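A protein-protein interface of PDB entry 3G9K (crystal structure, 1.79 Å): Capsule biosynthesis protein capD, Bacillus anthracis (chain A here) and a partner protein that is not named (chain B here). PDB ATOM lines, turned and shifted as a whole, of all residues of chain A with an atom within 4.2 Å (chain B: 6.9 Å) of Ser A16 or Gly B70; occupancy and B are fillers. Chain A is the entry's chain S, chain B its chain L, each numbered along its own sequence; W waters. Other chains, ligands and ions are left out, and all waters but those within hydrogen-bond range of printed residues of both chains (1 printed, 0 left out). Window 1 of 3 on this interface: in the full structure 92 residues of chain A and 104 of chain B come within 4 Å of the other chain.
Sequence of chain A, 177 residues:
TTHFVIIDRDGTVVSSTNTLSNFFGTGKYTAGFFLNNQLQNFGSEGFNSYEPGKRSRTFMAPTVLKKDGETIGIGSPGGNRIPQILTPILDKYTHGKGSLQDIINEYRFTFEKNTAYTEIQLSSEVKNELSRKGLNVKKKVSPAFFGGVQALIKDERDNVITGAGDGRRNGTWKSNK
Water W1 bridges the backbone carbonyl oxygen of Ser B52 (2.8 Å) and the side-chain amide nitrogen of Asn A18 (2.9 Å).
Printed residues of chain B that touch a printed residue of chain A: Ala B48, Ser B52, Gly B68, Gly B69, Gly B70, Met B71, Leu B72 and Tyr B84. Of the 8 printed residues of chain A, 6 touch a printed residue of chain B. Hydrophobic or aromatic side chains of chain A that line the printed part of chain B: Phe A4 and Val A14. Among the printed residues, 16 pairs touch across the chains. Among the printed residues, no Asp or Glu carboxylate lies within 4 Å of a Lys or Arg side-chain nitrogen of the other chain.
Among the printed residues, pairs that only touch across the chains: Thr A17 with Gly B69 (3.2 Å), Phe A4 with Ser B52 (3.3 Å), Val A14 with Leu B72 (3.3 Å), Asn A18 with Gly B68 (3.4 Å), Asn A18 with Gly B69 (3.6 Å), Val A14 with Met B71 (3.6 Å), Phe A4 with Ala B48 (3.7 Å), Ser A15 with Met B71 (3.9 Å), Ser A16 with Met B71 (3.9 Å) and Val A14 with Ala B48 (3.9 Å).
Printed residues of chain B within 4 Å of Ser A15: Met B71 and Leu B72. Ser A16 touches just these residues of chain B: Gly B70 (3.1 Å), Met B71 (3.9 Å) and Tyr B84 (3.1 Å). Of the printed residues of chain A, Ser B52 touches Phe A4 and Asn A18. Of the printed residues of chain A, Gly B69 touches Thr A17 (3.2 Å) and Asn A18 (3.6 Å). Gly B70 touches just these residues of chain A: Ser A16 and Thr A17. Printed residues of chain A within 4 Å of Met B71: Val A14 (3.6 Å), Ser A15 (3.9 Å) and Ser A16 (3.9 Å). The nearest residue of chain B that does not touch Ser A16 is Ser B52 (4.7 Å). The nearest residue of chain A that does not touch Gly B70 is Asn A18 (4.1 Å). The nearest printed residue of chain A that does not touch Met B71 is Phe A4 (4.3 Å).
O of Ala B48 lies within hydrogen-bond range of OG of Ser B52 (2.8 Å). The backbone NH (N) of Tyr B84 lies within hydrogen-bond range of the backbone carbonyl oxygen (O) of Gly B69 (3.0 Å). N of Ile B82 lies within hydrogen-bond range of O of Met B71, 2.8 Å away. The backbone NH (N) of Thr A2 is in hydrogen-bond range of the backbone carbonyl oxygen (O) of Asn A18, at 2.9 Å. NE2 of His A3 lies within hydrogen-bond range of OG of Ser A15. The backbone carbonyl oxygen (O) of Ser A16 sits close to a ring nitrogen (NE2) of His A3.
The side-chain amide nitrogen of Asn A18 lies within hydrogen-bond range of the side-chain hydroxyl of Ser B52 (3.2 Å). The backbone carbonyl oxygen of Gly B70 sits at hydrogen-bond distance from the side-chain hydroxyl of Ser A16 (3.1 Å). N of Gly B70 is in hydrogen-bond range of O of Thr A17. The backbone NH of Leu B72 is in hydrogen-bond range of the backbone carbonyl oxygen of Ser A15, at 2.9 Å. OH of Tyr B84 is in hydrogen-bond range of OG of Ser A16 (3.1 Å). OH of Tyr B84 lies within hydrogen-bond range of OD1 of Asn A18, 2.7 Å away.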
ATOM      1  N   THR A   2      -7.890  32.209  21.336  1.00  0.00           N
ATOM      2  CA  THR A   2      -7.389  31.757  22.643  1.00  0.00           C
ATOM      3  C   THR A   2      -6.951  30.326  22.453  1.00  0.00           C
ATOM      4  O   THR A   2      -7.607  29.600  21.718  1.00  0.00           O
ATOM      5  CB  THR A   2      -8.474  31.883  23.727  1.00  0.00           C
ATOM      6  OG1 THR A   2      -7.868  31.826  25.043  1.00  0.00           O
ATOM      7  CG2 THR A   2      -9.531  30.792  23.564  1.00  0.00           C
ATOM      8  N   HIS A   3      -5.835  29.943  23.091  1.00  0.00           N
ATOM      9  CA  HIS A   3      -5.376  28.589  23.071  1.00  0.00           C
ATOM     10  C   HIS A   3      -5.274  28.034  24.510  1.00  0.00           C
ATOM     11  O   HIS A   3      -4.703  28.708  25.369  1.00  0.00           O
ATOM     12  CB  HIS A   3      -4.043  28.449  22.436  1.00  0.00           C
ATOM     13  CG  HIS A   3      -3.724  27.033  22.174  1.00  0.00           C
ATOM     14  ND1 HIS A   3      -2.934  26.291  23.013  1.00  0.00           N
ATOM     15  CD2 HIS A   3      -4.189  26.183  21.242  1.00  0.00           C
ATOM     16  CE1 HIS A   3      -2.925  25.040  22.605  1.00  0.00           C
ATOM     17  NE2 HIS A   3      -3.664  24.957  21.519  1.00  0.00           N
ATOM     18  N   PHE A   4      -5.829  26.839  24.758  1.00  0.00           N
ATOM     19  CA  PHE A   4      -5.603  26.135  26.039  1.00  0.00           C
ATOM     20  C   PHE A   4      -5.129  24.662  25.843  1.00  0.00           C
ATOM     21  O   PHE A   4      -5.232  24.070  24.765  1.00  0.00           O
ATOM     22  CB  PHE A   4      -6.847  26.276  26.947  1.00  0.00           C
ATOM     23  CG  PHE A   4      -8.044  25.525  26.442  1.00  0.00           C
ATOM     24  CD1 PHE A   4      -8.914  26.123  25.558  1.00  0.00           C
ATOM     25  CD2 PHE A   4      -8.234  24.168  26.770  1.00  0.00           C
ATOM     26  CE1 PHE A   4     -10.013  25.446  25.077  1.00  0.00           C
ATOM     27  CE2 PHE A   4      -9.313  23.478  26.316  1.00  0.00           C
ATOM     28  CZ  PHE A   4     -10.215  24.110  25.444  1.00  0.00           C
ATOM     29  N   VAL A  14      -5.584  17.396  25.626  1.00  0.00           N
ATOM     30  CA  VAL A  14      -6.371  18.181  24.724  1.00  0.00           C
ATOM     31  C   VAL A  14      -5.595  19.470  24.432  1.00  0.00           C
ATOM     32  O   VAL A  14      -5.138  20.154  25.370  1.00  0.00           O
ATOM     33  CB  VAL A  14      -7.726  18.594  25.383  1.00  0.00           C
ATOM     34  CG1 VAL A  14      -8.432  19.658  24.532  1.00  0.00           C
ATOM     35  CG2 VAL A  14      -8.643  17.358  25.650  1.00  0.00           C
ATOM     36  N   SER A  15      -5.562  19.856  23.171  1.00  0.00           N
ATOM     37  CA  SER A  15      -4.972  21.139  22.767  1.00  0.00           C
ATOM     38  C   SER A  15      -6.003  21.789  21.873  1.00  0.00           C
ATOM     39  O   SER A  15      -6.315  21.248  20.787  1.00  0.00           O
ATOM     40  CB  SER A  15      -3.677  20.880  22.027  1.00  0.00           C
ATOM     41  OG  SER A  15      -2.960  22.050  21.765  1.00  0.00           O
ATOM     42  N   SER A  16      -6.533  22.931  22.302  1.00  0.00           N
ATOM     43  CA  SER A  16      -7.666  23.541  21.586  1.00  0.00           C
ATOM     44  C   SER A  16      -7.434  25.019  21.359  1.00  0.00           C
ATOM     45  O   SER A  16      -6.941  25.732  22.242  1.00  0.00           O
ATOM     46  CB  SER A  16      -8.964  23.280  22.328  1.00  0.00           C
ATOM     47  OG  SER A  16     -10.036  23.997  21.734  1.00  0.00           O
ATOM     48  N   THR A  17      -7.719  25.464  20.132  1.00  0.00           N
ATOM     49  CA  THR A  17      -7.787  26.908  19.875  1.00  0.00           C
ATOM     50  C   THR A  17      -9.154  27.373  19.342  1.00  0.00           C
ATOM     51  O   THR A  17      -9.695  26.838  18.396  1.00  0.00           O
ATOM     52  CB  THR A  17      -6.435  27.493  19.207  1.00  0.00           C
ATOM     53  OG1 THR A  17      -6.644  28.653  18.373  1.00  0.00           O
ATOM     54  CG2 THR A  17      -5.505  26.476  18.650  1.00  0.00           C
ATOM     55  N   ASN A  18      -9.743  28.334  20.049  1.00  0.00           N
ATOM     56  CA  ASN A  18     -11.040  28.870  19.724  1.00  0.00           C
ATOM     57  C   ASN A  18     -10.911  30.333  19.340  1.00  0.00           C
ATOM     58  O   ASN A  18      -9.997  31.016  19.808  1.00  0.00           O
ATOM     59  CB  ASN A  18     -11.972  28.765  20.915  1.00  0.00           C
ATOM     60  CG  ASN A  18     -12.234  27.306  21.343  1.00  0.00           C
ATOM     61  OD1 ASN A  18     -12.168  26.391  20.527  1.00  0.00           O
ATOM     62  ND2 ASN A  18     -12.551  27.111  22.624  1.00  0.00           N
ATOM     63  N   ALA B  48     -12.189  20.501  29.177  1.00  0.00           N
ATOM     64  CA  ALA B  48     -12.020  21.359  27.994  1.00  0.00           C
ATOM     65  C   ALA B  48     -13.344  22.070  27.609  1.00  0.00           C
ATOM     66  O   ALA B  48     -13.351  23.221  27.184  1.00  0.00           O
ATOM     67  CB  ALA B  48     -11.509  20.509  26.794  1.00  0.00           C
ATOM     68  N   SER B  52     -13.690  25.915  27.734  1.00  0.00           N
ATOM     69  CA  SER B  52     -14.069  26.655  26.490  1.00  0.00           C
ATOM     70  C   SER B  52     -15.218  27.614  26.744  1.00  0.00           C
ATOM     71  O   SER B  52     -15.159  28.795  26.391  1.00  0.00           O
ATOM     72  CB  SER B  52     -14.433  25.731  25.360  1.00  0.00           C
ATOM     73  OG  SER B  52     -13.306  25.012  24.970  1.00  0.00           O
ATOM     74  N   GLY B  68     -15.950  29.952  16.630  1.00  0.00           N
ATOM     75  CA  GLY B  68     -15.617  28.589  16.278  1.00  0.00           C
ATOM     76  C   GLY B  68     -14.285  28.210  16.849  1.00  0.00           C
ATOM     77  O   GLY B  68     -13.739  28.938  17.652  1.00  0.00           O
ATOM     78  N   GLY B  69     -13.730  27.091  16.395  1.00  0.00           N
ATOM     79  CA  GLY B  69     -12.522  26.576  16.990  1.00  0.00           C
ATOM     80  C   GLY B  69     -12.203  25.208  16.443  1.00  0.00           C
ATOM     81  O   GLY B  69     -12.937  24.683  15.563  1.00  0.00           O
ATOM     82  N   GLY B  70     -11.162  24.637  17.008  1.00  0.00           N
ATOM     83  CA  GLY B  70     -10.735  23.302  16.743  1.00  0.00           C
ATOM     84  C   GLY B  70     -10.103  22.701  17.970  1.00  0.00           C
ATOM     85  O   GLY B  70      -9.496  23.394  18.715  1.00  0.00           O
ATOM     86  N   MET B  71     -10.318  21.374  18.101  1.00  0.00           N
ATOM     87  CA  MET B  71      -9.827  20.673  19.272  1.00  0.00           C
ATOM     88  C   MET B  71      -9.152  19.376  18.897  1.00  0.00           C
ATOM     89  O   MET B  71      -9.752  18.488  18.253  1.00  0.00           O
ATOM     90  CB  MET B  71     -10.965  20.394  20.258  1.00  0.00           C
ATOM     91  CG  MET B  71     -10.507  19.704  21.560  1.00  0.00           C
ATOM     92  SD  MET B  71     -11.880  19.412  22.888  1.00  0.00           S
ATOM     93  CE  MET B  71     -12.427  21.277  23.153  1.00  0.00           C
ATOM     94  N   LEU B  72      -7.913  19.244  19.356  1.00  0.00           N
ATOM     95  CA  LEU B  72      -7.125  18.043  19.178  1.00  0.00           C
ATOM     96  C   LEU B  72      -7.231  17.265  20.465  1.00  0.00           C
ATOM     97  O   LEU B  72      -7.094  17.848  21.565  1.00  0.00           O
ATOM     98  CB  LEU B  72      -5.668  18.440  18.838  1.00  0.00           C
ATOM     99  CG  LEU B  72      -4.651  17.412  18.379  1.00  0.00           C
ATOM    100  CD1 LEU B  72      -5.103  16.782  17.087  1.00  0.00           C
ATOM    101  CD2 LEU B  72      -3.247  18.087  18.246  1.00  0.00           C
ATOM    102  N   PHE B  81      -9.325  14.969  15.792  1.00  0.00           N
ATOM    103  CA  PHE B  81      -9.413  16.409  15.629  1.00  0.00           C
ATOM    104  C   PHE B  81     -10.873  16.798  15.350  1.00  0.00           C
ATOM    105  O   PHE B  81     -11.470  16.300  14.413  1.00  0.00           O
ATOM    106  CB  PHE B  81      -8.530  16.934  14.487  1.00  0.00           C
ATOM    107  CG  PHE B  81      -8.531  18.427  14.414  1.00  0.00           C
ATOM    108  CD1 PHE B  81      -7.714  19.162  15.252  1.00  0.00           C
ATOM    109  CD2 PHE B  81      -9.402  19.096  13.592  1.00  0.00           C
ATOM    110  CE1 PHE B  81      -7.748  20.553  15.241  1.00  0.00           C
ATOM    111  CE2 PHE B  81      -9.432  20.490  13.583  1.00  0.00           C
ATOM    112  CZ  PHE B  81      -8.584  21.201  14.407  1.00  0.00           C
ATOM    113  N   ILE B  82     -11.471  17.637  16.192  1.00  0.00           N
ATOM    114  CA  ILE B  82     -12.816  18.116  15.899  1.00  0.00           C
ATOM    115  C   ILE B  82     -12.780  19.574  15.363  1.00  0.00           C
ATOM    116  O   ILE B  82     -12.292  20.488  16.028  1.00  0.00           O
ATOM    117  CB  ILE B  82     -13.742  18.021  17.101  1.00  0.00           C
ATOM    118  CG1 ILE B  82     -13.578  16.677  17.806  1.00  0.00           C
ATOM    119  CG2 ILE B  82     -15.181  18.294  16.651  1.00  0.00           C
ATOM    120  CD1 ILE B  82     -13.669  15.513  16.863  1.00  0.00           C
ATOM    121  N   ASP B  83     -13.280  19.741  14.147  1.00  0.00           N
ATOM    122  CA  ASP B  83     -13.348  21.008  13.454  1.00  0.00           C
ATOM    123  C   ASP B  83     -14.739  21.635  13.653  1.00  0.00           C
ATOM    124  O   ASP B  83     -15.723  21.191  13.046  1.00  0.00           O
ATOM    125  CB  ASP B  83     -13.071  20.775  11.956  1.00  0.00           C
ATOM    126  CG  ASP B  83     -13.078  22.083  11.140  1.00  0.00           C
ATOM    127  OD1 ASP B  83     -13.615  23.111  11.614  1.00  0.00           O
ATOM    128  OD2 ASP B  83     -12.497  22.117  10.038  1.00  0.00           O
ATOM    129  N   TYR B  84     -14.818  22.677  14.483  1.00  0.00           N
ATOM    130  CA  TYR B  84     -16.062  23.435  14.666  1.00  0.00           C
ATOM    131  C   TYR B  84     -15.874  24.923  14.271  1.00  0.00           C
ATOM    132  O   TYR B  84     -16.417  25.848  14.868  1.00  0.00           O
ATOM    133  CB  TYR B  84     -16.619  23.248  16.092  1.00  0.00           C
ATOM    134  CG  TYR B  84     -15.563  23.408  17.199  1.00  0.00           C
ATOM    135  CD1 TYR B  84     -15.411  24.597  17.877  1.00  0.00           C
ATOM    136  CD2 TYR B  84     -14.731  22.364  17.539  1.00  0.00           C
ATOM    137  CE1 TYR B  84     -14.452  24.735  18.849  1.00  0.00           C
ATOM    138  CE2 TYR B  84     -13.770  22.498  18.490  1.00  0.00           C
ATOM    139  CZ  TYR B  84     -13.646  23.684  19.172  1.00  0.00           C
ATOM    140  OH  TYR B  84     -12.657  23.799  20.127  1.00  0.00           O
ATOM    141  N   ARG B  85     -15.145  25.110  13.183  1.00  0.00           N
ATOM    142  CA  ARG B  85     -14.957  26.380  12.601  1.00  0.00           C
ATOM    143  C   ARG B  85     -16.270  26.797  11.943  1.00  0.00           C
ATOM    144  O   ARG B  85     -17.029  25.937  11.464  1.00  0.00           O
ATOM    145  CB  ARG B  85     -13.832  26.261  11.578  1.00  0.00           C
ATOM    146  CG  ARG B  85     -13.357  27.552  11.033  1.00  0.00           C
ATOM    147  CD  ARG B  85     -11.936  27.406  10.466  1.00  0.00           C
ATOM    148  NE  ARG B  85     -11.530  28.618   9.762  1.00  0.00           N
ATOM    149  CZ  ARG B  85     -11.199  29.756  10.362  1.00  0.00           C
ATOM    150  NH1 ARG B  85     -11.224  29.876  11.690  1.00  0.00           N
ATOM    151  NH2 ARG B  85     -10.827  30.791   9.622  1.00  0.00           N
ATOM    152  N   MET B 108     -18.900  21.811  20.911  1.00  0.00           N
ATOM    153  CA  MET B 108     -18.896  21.372  22.303  1.00  0.00           C
ATOM    154  C   MET B 108     -19.905  20.247  22.532  1.00  0.00           C
ATOM    155  O   MET B 108     -19.594  19.262  23.228  1.00  0.00           O
ATOM    156  CB  MET B 108     -19.184  22.548  23.247  1.00  0.00           C
ATOM    157  CG  MET B 108     -18.115  23.660  23.244  1.00  0.00           C
ATOM    158  SD  MET B 108     -16.315  23.015  23.613  1.00  0.00           S
ATOM    159  CE  MET B 108     -15.390  23.523  22.016  1.00  0.00           C
ATOM    160  N   ILE B 111     -18.475  17.063  20.795  1.00  0.00           N
ATOM    161  CA  ILE B 111     -17.368  16.623  21.634  1.00  0.00           C
ATOM    162  C   ILE B 111     -17.888  15.948  22.874  1.00  0.00           C
ATOM    163  O   ILE B 111     -17.454  14.878  23.233  1.00  0.00           O
ATOM    164  CB  ILE B 111     -16.459  17.830  22.015  1.00  0.00           C
ATOM    165  CG1 ILE B 111     -15.710  18.267  20.740  1.00  0.00           C
ATOM    166  CG2 ILE B 111     -15.488  17.464  23.206  1.00  0.00           C
ATOM    167  CD1 ILE B 111     -14.994  19.689  20.772  1.00  0.00           C
ATOM    168  N   PHE B 240      -7.087  23.952   8.897  1.00  0.00           N
ATOM    169  CA  PHE B 240      -6.120  24.470   9.890  1.00  0.00           C
ATOM    170  C   PHE B 240      -4.710  24.346   9.285  1.00  0.00           C
ATOM    171  O   PHE B 240      -4.545  23.716   8.228  1.00  0.00           O
ATOM    172  CB  PHE B 240      -6.238  23.705  11.213  1.00  0.00           C
ATOM    173  CG  PHE B 240      -7.508  24.019  12.001  1.00  0.00           C
ATOM    174  CD1 PHE B 240      -7.440  24.783  13.149  1.00  0.00           C
ATOM    175  CD2 PHE B 240      -8.751  23.552  11.577  1.00  0.00           C
ATOM    176  CE1 PHE B 240      -8.591  25.078  13.888  1.00  0.00           C
ATOM    177  CE2 PHE B 240      -9.923  23.844  12.293  1.00  0.00           C
ATOM    178  CZ  PHE B 240      -9.835  24.614  13.446  1.00  0.00           C
HETATM  179  O   HOH W   1     -13.323  29.262  24.343  1.00  0.00           O
